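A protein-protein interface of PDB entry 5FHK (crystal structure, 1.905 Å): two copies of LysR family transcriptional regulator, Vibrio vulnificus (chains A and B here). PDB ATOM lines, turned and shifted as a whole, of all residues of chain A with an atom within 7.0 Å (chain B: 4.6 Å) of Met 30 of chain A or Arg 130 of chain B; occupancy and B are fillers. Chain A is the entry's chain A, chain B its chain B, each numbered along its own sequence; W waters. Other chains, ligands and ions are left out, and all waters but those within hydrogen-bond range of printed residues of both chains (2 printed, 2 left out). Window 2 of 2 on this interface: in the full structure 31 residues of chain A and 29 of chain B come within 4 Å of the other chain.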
ATOM      1  N   MET A  23     -20.147  15.623  24.346  1.00  0.00           N
ATOM      2  CA  MET A  23     -19.892  16.521  25.471  1.00  0.00           C
ATOM      3  C   MET A  23     -19.322  15.844  26.716  1.00  0.00           C
ATOM      4  O   MET A  23     -18.555  16.507  27.434  1.00  0.00           O
ATOM      5  CB  MET A  23     -21.183  17.285  25.846  1.00  0.00           C
ATOM      6  CG  MET A  23     -21.454  18.556  25.023  1.00  0.00           C
ATOM      7  SD  MET A  23     -19.997  19.485  24.436  1.00  0.00           S
ATOM      8  CE  MET A  23     -19.462  20.329  25.932  1.00  0.00           C
ATOM      9  N   MET A  25     -17.104  13.428  26.927  1.00  0.00           N
ATOM     10  CA  MET A  25     -15.681  13.377  26.616  1.00  0.00           C
ATOM     11  C   MET A  25     -15.076  14.769  26.588  1.00  0.00           C
ATOM     12  O   MET A  25     -13.995  15.000  27.147  1.00  0.00           O
ATOM     13  CB  MET A  25     -15.498  12.713  25.261  1.00  0.00           C
ATOM     14  CG  MET A  25     -14.104  12.262  24.926  1.00  0.00           C
ATOM     15  SD  MET A  25     -14.332  10.949  23.658  1.00  0.00           S
ATOM     16  CE  MET A  25     -15.607  11.658  22.615  1.00  0.00           C
ATOM     17  N   LEU A  26     -15.758  15.712  25.930  1.00  0.00           N
ATOM     18  CA  LEU A  26     -15.210  17.062  25.808  1.00  0.00           C
ATOM     19  C   LEU A  26     -15.124  17.750  27.156  1.00  0.00           C
ATOM     20  O   LEU A  26     -14.186  18.513  27.407  1.00  0.00           O
ATOM     21  CB  LEU A  26     -16.069  17.890  24.856  1.00  0.00           C
ATOM     22  CG  LEU A  26     -15.781  17.515  23.405  1.00  0.00           C
ATOM     23  CD1 LEU A  26     -16.885  18.037  22.511  1.00  0.00           C
ATOM     24  CD2 LEU A  26     -14.433  18.094  23.005  1.00  0.00           C
ATOM     25  N   ASN A  27     -16.124  17.557  28.009  1.00  0.00           N
ATOM     26  CA  ASN A  27     -16.071  18.212  29.317  1.00  0.00           C
ATOM     27  C   ASN A  27     -14.969  17.597  30.176  1.00  0.00           C
ATOM     28  O   ASN A  27     -14.256  18.313  30.891  1.00  0.00           O
ATOM     29  CB  ASN A  27     -17.445  18.129  30.019  1.00  0.00           C
ATOM     30  CG  ASN A  27     -18.479  19.092  29.446  1.00  0.00           C
ATOM     31  OD1 ASN A  27     -18.123  20.163  28.925  1.00  0.00           O
ATOM     32  ND2 ASN A  27     -19.784  18.728  29.553  1.00  0.00           N
ATOM     33  N   GLY A  28     -14.748  16.290  30.052  1.00  0.00           N
ATOM     34  CA  GLY A  28     -13.654  15.673  30.789  1.00  0.00           C
ATOM     35  C   GLY A  28     -12.301  16.140  30.296  1.00  0.00           C
ATOM     36  O   GLY A  28     -11.369  16.307  31.083  1.00  0.00           O
ATOM     37  N   PHE A  29     -12.177  16.390  28.994  1.00  0.00           N
ATOM     38  CA  PHE A  29     -10.901  16.848  28.481  1.00  0.00           C
ATOM     39  C   PHE A  29     -10.609  18.262  28.957  1.00  0.00           C
ATOM     40  O   PHE A  29      -9.499  18.558  29.420  1.00  0.00           O
ATOM     41  CB  PHE A  29     -10.896  16.771  26.960  1.00  0.00           C
ATOM     42  CG  PHE A  29      -9.710  17.438  26.333  1.00  0.00           C
ATOM     43  CD1 PHE A  29      -8.506  16.780  26.242  1.00  0.00           C
ATOM     44  CD2 PHE A  29      -9.787  18.748  25.896  1.00  0.00           C
ATOM     45  CE1 PHE A  29      -7.427  17.395  25.676  1.00  0.00           C
ATOM     46  CE2 PHE A  29      -8.697  19.377  25.324  1.00  0.00           C
ATOM     47  CZ  PHE A  29      -7.516  18.704  25.211  1.00  0.00           C
ATOM     48  N   MET A  30     -11.596  19.152  28.829  1.00  0.00           N
ATOM     49  CA  MET A  30     -11.412  20.539  29.242  1.00  0.00           C
ATOM     50  C   MET A  30     -11.098  20.613  30.720  1.00  0.00           C
ATOM     51  O   MET A  30     -10.365  21.501  31.173  1.00  0.00           O
ATOM     52  CB  MET A  30     -12.674  21.349  28.944  1.00  0.00           C
ATOM     53  CG  MET A  30     -12.898  21.605  27.448  1.00  0.00           C
ATOM     54  SD  MET A  30     -14.153  22.858  27.137  1.00  0.00           S
ATOM     55  CE  MET A  30     -15.658  21.895  27.158  1.00  0.00           C
ATOM     56  N   SER A  31     -11.722  19.727  31.480  1.00  0.00           N
ATOM     57  CA  SER A  31     -11.472  19.611  32.895  1.00  0.00           C
ATOM     58  C   SER A  31     -10.010  19.284  33.160  1.00  0.00           C
ATOM     59  O   SER A  31      -9.399  19.857  34.063  1.00  0.00           O
ATOM     60  CB  SER A  31     -12.396  18.533  33.452  1.00  0.00           C
ATOM     61  OG  SER A  31     -12.684  18.768  34.783  1.00  0.00           O
ATOM     62  N   GLN A  32      -9.417  18.399  32.344  1.00  0.00           N
ATOM     63  CA  GLN A  32      -8.049  17.962  32.580  1.00  0.00           C
ATOM     64  C   GLN A  32      -7.020  18.957  32.046  1.00  0.00           C
ATOM     65  O   GLN A  32      -5.892  18.998  32.553  1.00  0.00           O
ATOM     66  CB  GLN A  32      -7.843  16.576  31.946  1.00  0.00           C
ATOM     67  CG  GLN A  32      -6.584  15.818  32.376  1.00  0.00           C
ATOM     68  CD  GLN A  32      -6.533  14.409  31.794  1.00  0.00           C
ATOM     69  OE1 GLN A  32      -7.519  13.660  31.841  1.00  0.00           O
ATOM     70  NE2 GLN A  32      -5.387  14.046  31.220  1.00  0.00           N
ATOM     71  N   TYR A  33      -7.388  19.761  31.044  1.00  0.00           N
ATOM     72  CA  TYR A  33      -6.484  20.714  30.403  1.00  0.00           C
ATOM     73  C   TYR A  33      -7.150  22.082  30.385  1.00  0.00           C
ATOM     74  O   TYR A  33      -7.536  22.589  29.326  1.00  0.00           O
ATOM     75  CB  TYR A  33      -6.124  20.259  28.992  1.00  0.00           C
ATOM     76  CG  TYR A  33      -5.475  18.904  28.953  1.00  0.00           C
ATOM     77  CD1 TYR A  33      -4.138  18.749  29.243  1.00  0.00           C
ATOM     78  CD2 TYR A  33      -6.211  17.777  28.677  1.00  0.00           C
ATOM     79  CE1 TYR A  33      -3.553  17.504  29.205  1.00  0.00           C
ATOM     80  CE2 TYR A  33      -5.639  16.539  28.633  1.00  0.00           C
ATOM     81  CZ  TYR A  33      -4.306  16.401  28.892  1.00  0.00           C
ATOM     82  OH  TYR A  33      -3.735  15.149  28.864  1.00  0.00           O
ATOM     83  N   PRO A  34      -7.303  22.708  31.554  1.00  0.00           N
ATOM     84  CA  PRO A  34      -7.915  24.052  31.600  1.00  0.00           C
ATOM     85  C   PRO A  34      -7.187  25.093  30.766  1.00  0.00           C
ATOM     86  O   PRO A  34      -7.797  26.100  30.385  1.00  0.00           O
ATOM     87  CB  PRO A  34      -7.853  24.412  33.088  1.00  0.00           C
ATOM     88  CG  PRO A  34      -7.513  23.135  33.794  1.00  0.00           C
ATOM     89  CD  PRO A  34      -6.748  22.309  32.855  1.00  0.00           C
ATOM     90  N   GLU A  35      -5.887  24.905  30.504  1.00  0.00           N
ATOM     91  CA  GLU A  35      -5.127  25.846  29.693  1.00  0.00           C
ATOM     92  C   GLU A  35      -5.484  25.771  28.212  1.00  0.00           C
ATOM     93  O   GLU A  35      -5.155  26.696  27.469  1.00  0.00           O
ATOM     94  CB  GLU A  35      -3.628  25.598  29.879  1.00  0.00           C
ATOM     95  CG  GLU A  35      -3.163  24.215  29.424  1.00  0.00           C
ATOM     96  CD  GLU A  35      -3.418  23.115  30.451  1.00  0.00           C
ATOM     97  OE1 GLU A  35      -3.966  23.393  31.541  1.00  0.00           O
ATOM     98  OE2 GLU A  35      -3.074  21.955  30.164  1.00  0.00           O
ATOM     99  N   ILE A  36      -6.153  24.704  27.769  1.00  0.00           N
ATOM    100  CA  ILE A  36      -6.481  24.511  26.361  1.00  0.00           C
ATOM    101  C   ILE A  36      -7.870  25.063  26.078  1.00  0.00           C
ATOM    102  O   ILE A  36      -8.812  24.833  26.855  1.00  0.00           O
ATOM    103  CB  ILE A  36      -6.390  23.017  25.998  1.00  0.00           C
ATOM    104  CG1 ILE A  36      -4.953  22.516  26.228  1.00  0.00           C
ATOM    105  CG2 ILE A  36      -6.862  22.764  24.569  1.00  0.00           C
ATOM    106  CD1 ILE A  36      -4.743  21.062  25.818  1.00  0.00           C
ATOM    107  N   ASN A  37      -8.002  25.803  24.977  1.00  0.00           N
ATOM    108  CA  ASN A  37      -9.288  26.349  24.545  1.00  0.00           C
ATOM    109  C   ASN A  37      -9.846  25.537  23.384  1.00  0.00           C
ATOM    110  O   ASN A  37      -9.092  25.092  22.507  1.00  0.00           O
ATOM    111  CB  ASN A  37      -9.168  27.821  24.120  1.00  0.00           C
ATOM    112  CG  ASN A  37      -8.595  28.721  25.219  1.00  0.00           C
ATOM    113  OD1 ASN A  37      -9.069  28.724  26.360  1.00  0.00           O
ATOM    114  ND2 ASN A  37      -7.558  29.491  24.872  1.00  0.00           N
ATOM    115  N   ILE A  38     -11.176  25.391  23.354  1.00  0.00           N
ATOM    116  CA  ILE A  38     -11.887  24.660  22.307  1.00  0.00           C
ATOM    117  C   ILE A  38     -12.864  25.593  21.603  1.00  0.00           C
ATOM    118  O   ILE A  38     -13.586  26.350  22.258  1.00  0.00           O
ATOM    119  CB  ILE A  38     -12.662  23.455  22.876  1.00  0.00           C
ATOM    120  CG1 ILE A  38     -11.722  22.514  23.615  1.00  0.00           C
ATOM    121  CG2 ILE A  38     -13.435  22.742  21.750  1.00  0.00           C
ATOM    122  CD1 ILE A  38     -11.029  21.557  22.705  1.00  0.00           C
ATOM    123  N   GLU A  39     -12.889  25.532  20.274  1.00  0.00           N
ATOM    124  CA  GLU A  39     -13.959  26.106  19.462  1.00  0.00           C
ATOM    125  C   GLU A  39     -14.650  24.949  18.759  1.00  0.00           C
ATOM    126  O   GLU A  39     -13.987  24.167  18.063  1.00  0.00           O
ATOM    127  CB  GLU A  39     -13.432  27.116  18.424  1.00  0.00           C
ATOM    128  CG  GLU A  39     -13.199  28.529  18.986  1.00  0.00           C
ATOM    129  CD  GLU A  39     -12.865  29.555  17.900  1.00  0.00           C
ATOM    130  OE1 GLU A  39     -12.964  29.199  16.697  1.00  0.00           O
ATOM    131  OE2 GLU A  39     -12.476  30.705  18.249  1.00  0.00           O
ATOM    132  N   PHE A 197      -5.397  16.254  22.714  1.00  0.00           N
ATOM    133  CA  PHE A 197      -6.828  16.017  22.610  1.00  0.00           C
ATOM    134  C   PHE A 197      -7.094  14.642  22.022  1.00  0.00           C
ATOM    135  O   PHE A 197      -7.862  13.854  22.578  1.00  0.00           O
ATOM    136  CB  PHE A 197      -7.476  17.115  21.764  1.00  0.00           C
ATOM    137  CG  PHE A 197      -8.923  16.909  21.536  1.00  0.00           C
ATOM    138  CD1 PHE A 197      -9.828  17.086  22.561  1.00  0.00           C
ATOM    139  CD2 PHE A 197      -9.392  16.504  20.298  1.00  0.00           C
ATOM    140  CE1 PHE A 197     -11.180  16.874  22.335  1.00  0.00           C
ATOM    141  CE2 PHE A 197     -10.714  16.291  20.079  1.00  0.00           C
ATOM    142  CZ  PHE A 197     -11.615  16.478  21.082  1.00  0.00           C
ATOM    143  N   TYR A 200      -6.469  11.883  24.458  1.00  0.00           N
ATOM    144  CA  TYR A 200      -7.548  11.812  25.439  1.00  0.00           C
ATOM    145  C   TYR A 200      -8.727  11.023  24.880  1.00  0.00           C
ATOM    146  O   TYR A 200      -9.247  10.115  25.539  1.00  0.00           O
ATOM    147  CB  TYR A 200      -7.990  13.213  25.860  1.00  0.00           C
ATOM    148  CG  TYR A 200      -8.975  13.184  27.015  1.00  0.00           C
ATOM    149  CD1 TYR A 200      -8.533  13.129  28.346  1.00  0.00           C
ATOM    150  CD2 TYR A 200     -10.338  13.177  26.779  1.00  0.00           C
ATOM    151  CE1 TYR A 200      -9.444  13.091  29.401  1.00  0.00           C
ATOM    152  CE2 TYR A 200     -11.232  13.154  27.809  1.00  0.00           C
ATOM    153  CZ  TYR A 200     -10.789  13.109  29.113  1.00  0.00           C
ATOM    154  OH  TYR A 200     -11.736  13.078  30.091  1.00  0.00           O
ATOM    155  N   PHE B 103     -12.520  31.906  33.465  1.00  0.00           N
ATOM    156  CA  PHE B 103     -12.835  31.083  32.305  1.00  0.00           C
ATOM    157  C   PHE B 103     -14.215  31.460  31.782  1.00  0.00           C
ATOM    158  O   PHE B 103     -15.180  31.465  32.547  1.00  0.00           O
ATOM    159  CB  PHE B 103     -12.825  29.597  32.673  1.00  0.00           C
ATOM    160  CG  PHE B 103     -11.484  29.072  33.119  1.00  0.00           C
ATOM    161  CD1 PHE B 103     -10.510  28.734  32.191  1.00  0.00           C
ATOM    162  CD2 PHE B 103     -11.208  28.886  34.470  1.00  0.00           C
ATOM    163  CE1 PHE B 103      -9.280  28.209  32.597  1.00  0.00           C
ATOM    164  CE2 PHE B 103      -9.958  28.371  34.891  1.00  0.00           C
ATOM    165  CZ  PHE B 103      -9.007  28.032  33.947  1.00  0.00           C
ATOM    166  N   LEU B 104     -14.310  31.765  30.489  1.00  0.00           N
ATOM    167  CA  LEU B 104     -15.562  32.114  29.836  1.00  0.00           C
ATOM    168  C   LEU B 104     -16.010  30.979  28.920  1.00  0.00           C
ATOM    169  O   LEU B 104     -15.193  30.269  28.323  1.00  0.00           O
ATOM    170  CB  LEU B 104     -15.396  33.403  29.033  1.00  0.00           C
ATOM    171  CG  LEU B 104     -15.040  34.624  29.908  1.00  0.00           C
ATOM    172  CD1 LEU B 104     -15.282  36.002  29.206  1.00  0.00           C
ATOM    173  CD2 LEU B 104     -15.718  34.596  31.275  1.00  0.00           C
ATOM    174  N   LEU B 105     -17.320  30.813  28.813  1.00  0.00           N
ATOM    175  CA  LEU B 105     -17.931  29.823  27.943  1.00  0.00           C
ATOM    176  C   LEU B 105     -18.967  30.550  27.104  1.00  0.00           C
ATOM    177  O   LEU B 105     -19.883  31.166  27.657  1.00  0.00           O
ATOM    178  CB  LEU B 105     -18.574  28.709  28.770  1.00  0.00           C
ATOM    179  CG  LEU B 105     -17.805  28.219  30.015  1.00  0.00           C
ATOM    180  CD1 LEU B 105     -18.662  27.232  30.826  1.00  0.00           C
ATOM    181  CD2 LEU B 105     -16.530  27.534  29.605  1.00  0.00           C
ATOM    182  N   ARG B 128     -11.463  35.441  24.409  1.00  0.00           N
ATOM    183  CA  ARG B 128     -11.662  34.124  23.823  1.00  0.00           C
ATOM    184  C   ARG B 128     -12.080  33.148  24.916  1.00  0.00           C
ATOM    185  O   ARG B 128     -11.374  32.981  25.918  1.00  0.00           O
ATOM    186  CB  ARG B 128     -10.394  33.650  23.127  1.00  0.00           C
ATOM    187  CG  ARG B 128     -10.525  32.294  22.483  1.00  0.00           C
ATOM    188  CD  ARG B 128      -9.279  31.503  22.784  1.00  0.00           C
ATOM    189  NE  ARG B 128      -8.090  32.301  22.500  1.00  0.00           N
ATOM    190  CZ  ARG B 128      -7.485  32.330  21.318  1.00  0.00           C
ATOM    191  NH1 ARG B 128      -7.956  31.585  20.320  1.00  0.00           N
ATOM    192  NH2 ARG B 128      -6.404  33.085  21.137  1.00  0.00           N
ATOM    193  N   GLY B 129     -13.238  32.520  24.734  1.00  0.00           N
ATOM    194  CA  GLY B 129     -13.730  31.601  25.738  1.00  0.00           C
ATOM    195  C   GLY B 129     -12.838  30.383  25.879  1.00  0.00           C
ATOM    196  O   GLY B 129     -12.164  29.949  24.942  1.00  0.00           O
ATOM    197  N   ARG B 130     -12.824  29.830  27.088  1.00  0.00           N
ATOM    198  CA  ARG B 130     -12.331  28.472  27.255  1.00  0.00           C
ATOM    199  C   ARG B 130     -13.018  27.534  26.273  1.00  0.00           C
ATOM    200  O   ARG B 130     -12.408  26.609  25.733  1.00  0.00           O
ATOM    201  CB  ARG B 130     -12.578  28.013  28.690  1.00  0.00           C
ATOM    202  CG  ARG B 130     -12.042  26.637  29.008  1.00  0.00           C
ATOM    203  CD  ARG B 130     -12.534  26.179  30.365  1.00  0.00           C
ATOM    204  NE  ARG B 130     -11.776  25.034  30.867  1.00  0.00           N
ATOM    205  CZ  ARG B 130     -11.760  24.671  32.144  1.00  0.00           C
ATOM    206  NH1 ARG B 130     -12.496  25.371  33.021  1.00  0.00           N
ATOM    207  NH2 ARG B 130     -11.037  23.603  32.548  1.00  0.00           N
ATOM    208  N   PHE B 131     -14.295  27.778  26.016  1.00  0.00           N
ATOM    209  CA  PHE B 131     -15.098  26.924  25.165  1.00  0.00           C
ATOM    210  C   PHE B 131     -15.983  27.848  24.348  1.00  0.00           C
ATOM    211  O   PHE B 131     -16.683  28.693  24.917  1.00  0.00           O
ATOM    212  CB  PHE B 131     -15.921  25.946  26.019  1.00  0.00           C
ATOM    213  CG  PHE B 131     -16.762  24.979  25.233  1.00  0.00           C
ATOM    214  CD1 PHE B 131     -16.201  24.144  24.290  1.00  0.00           C
ATOM    215  CD2 PHE B 131     -18.129  24.877  25.476  1.00  0.00           C
ATOM    216  CE1 PHE B 131     -16.989  23.231  23.577  1.00  0.00           C
ATOM    217  CE2 PHE B 131     -18.921  23.969  24.769  1.00  0.00           C
ATOM    218  CZ  PHE B 131     -18.355  23.148  23.823  1.00  0.00           C
ATOM    219  N   GLN B 132     -15.916  27.722  23.026  1.00  0.00           N
ATOM    220  CA  GLN B 132     -16.822  28.424  22.139  1.00  0.00           C
ATOM    221  C   GLN B 132     -17.529  27.405  21.268  1.00  0.00           C
ATOM    222  O   GLN B 132     -16.922  26.420  20.832  1.00  0.00           O
ATOM    223  CB  GLN B 132     -16.078  29.465  21.298  1.00  0.00           C
ATOM    224  CG  GLN B 132     -15.927  30.754  22.077  1.00  0.00           C
ATOM    225  CD  GLN B 132     -15.074  31.824  21.383  1.00  0.00           C
ATOM    226  OE1 GLN B 132     -14.322  32.549  22.048  1.00  0.00           O
ATOM    227  NE2 GLN B 132     -15.209  31.943  20.057  1.00  0.00           N
ATOM    228  N   ALA B 142     -21.341  22.557  29.427  1.00  0.00           N
ATOM    229  CA  ALA B 142     -20.008  22.851  29.960  1.00  0.00           C
ATOM    230  C   ALA B 142     -20.089  23.738  31.196  1.00  0.00           C
ATOM    231  O   ALA B 142     -19.321  23.566  32.146  1.00  0.00           O
ATOM    232  CB  ALA B 142     -19.127  23.505  28.890  1.00  0.00           C
ATOM    233  N   LEU B 147     -16.975  24.552  34.348  1.00  0.00           N
ATOM    234  CA  LEU B 147     -15.826  24.991  33.579  1.00  0.00           C
ATOM    235  C   LEU B 147     -15.797  26.499  33.373  1.00  0.00           C
ATOM    236  O   LEU B 147     -14.911  26.990  32.683  1.00  0.00           O
ATOM    237  CB  LEU B 147     -15.796  24.276  32.225  1.00  0.00           C
ATOM    238  CG  LEU B 147     -15.809  22.739  32.398  1.00  0.00           C
ATOM    239  CD1 LEU B 147     -16.104  22.056  31.083  1.00  0.00           C
ATOM    240  CD2 LEU B 147     -14.439  22.243  32.955  1.00  0.00           C
HETATM  241  O   HOH W   1     -10.794  22.583  35.375  1.00  0.00           O
HETATM  242  O   HOH W   2     -12.308  28.976  22.542  1.00  0.00           O
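The backbone carbonyl oxygen of Met 30 of chain A sits at hydrogen-bond distance from the guanidinium group of Arg 130 of chain B (2.6 Å).
The backbone NH of Ile 38 of chain A is in hydrogen-bond range of the backbone carbonyl oxygen of Arg 130 of chain B, at 2.9 Å.
The backbone carbonyl oxygen of Ile 38 of chain A lies within hydrogen-bond range of the backbone NH of Gln 132 of chain B (2.8 Å).
Water W2 lies within hydrogen-bond range of the backbone carbonyl oxygen (O) of Gly 129 of chain B (2.6 Å) and the backbone carbonyl oxygen (O) of Ile 38 of chain A (2.9 Å).
Water W1 bridges NH2 of Arg 130 of chain B (3.0 Å) and O of Ser 31 of chain A (3.3 Å).
Hydrophobic or aromatic side chains of chain A within 4 Å of the printed part of chain B: Met 23, Met 30, Pro 34 and Ile 38.
Of the 10 printed residues of chain B, 8 touch a printed residue of chain A.
Hydrophobic or aromatic side chains of chain B that line the printed part of chain A: Phe 103, Phe 131, Ala 142 and Leu 147.
Among the printed residues, no Asp or Glu carboxylate lies within 4 Å of a Lys or Arg side-chain nitrogen of the other chain.
Of chain B, only Arg 130, Phe 131 and Leu 147 come within 4 Å of Met 30 of chain A.
Of chain A, only Met 30, Pro 34, Asn 37 and Ile 38 come within 4 Å of Arg 130 of chain B.
Of the printed residues of chain A, Ala 142 of chain B touches Asn 27 (3.4 Å).
Printed residues of chain A within 4 Å of Phe 131 of chain B: Met 23, Met 30 and Ile 38.
Of the printed residues of chain A, Leu 147 of chain B touches Asn 27 (3.5 Å), Met 30 (3.95 Å) and Ser 31 (3.97 Å).
Of the printed residues of chain B, Ser 31 of chain A touches Leu 147 (3.97 Å).
Met 25 of chain A touches none of the printed residues of chain B.
The nearest residue of chain B that does not touch Met 30 of chain A is Ala 142 of chain B (4.2 Å).
The nearest residue of chain A that does not touch Arg 130 of chain B is Ser 31 of chain A (4.03 Å).
Among the printed residues, pairs that only touch across the chains: Met 23 of chain A with Phe 131 of chain B (3.7 Å), Asn 27 of chain A with Ala 142 of chain B (3.4 Å), Asn 27 of chain A with Leu 147 of chain B (3.5 Å), Met 30 of chain A with Phe 131 of chain B (3.7 Å), Met 30 of chain A with Leu 147 of chain B (3.95 Å), Ser 31 of chain A with Leu 147 of chain B (3.97 Å), Pro 34 of chain A with Phe 103 of chain B (3.4 Å), Pro 34 of chain A with Arg 130 of chain B (3.3 Å), Asn 37 of chain A with Arg 128 of chain B (3.4 Å), Asn 37 of chain A with Gly 129 of chain B (3.6 Å), Asn 37 of chain A with Arg 130 of chain B (3.3 Å), Ile 38 of chain A with Phe 131 of chain B (3.3 Å) and Glu 39 of chain A with Gln 132 of chain B (3.3 Å).
No position is printed for both chains.
Of the 16 pairs that touch across the chains among the printed residues, none has its exchanged pair printed and touching as well.
O of Met 23 of chain A lies close to ND2 of Asn 27 of chain A (3.3 Å).
The backbone carbonyl oxygen of Leu 104 of chain B lies within hydrogen-bond range of the backbone NH of Arg 130 of chain B, at 2.7 Å.
The backbone NH (N) of Gly 129 of chain B lies within hydrogen-bond range of the side-chain amide oxygen (OE1) of Gln 132 of chain B (2.9 Å).
The guanidinium group (NH1) of Arg 130 of chain B is in hydrogen-bond range of the backbone carbonyl oxygen (O) of Leu 147 of chain B (2.9 Å).
O of Ala 142 of chain B sits at hydrogen-bond distance from N of Leu 147 of chain B (3.4 Å).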
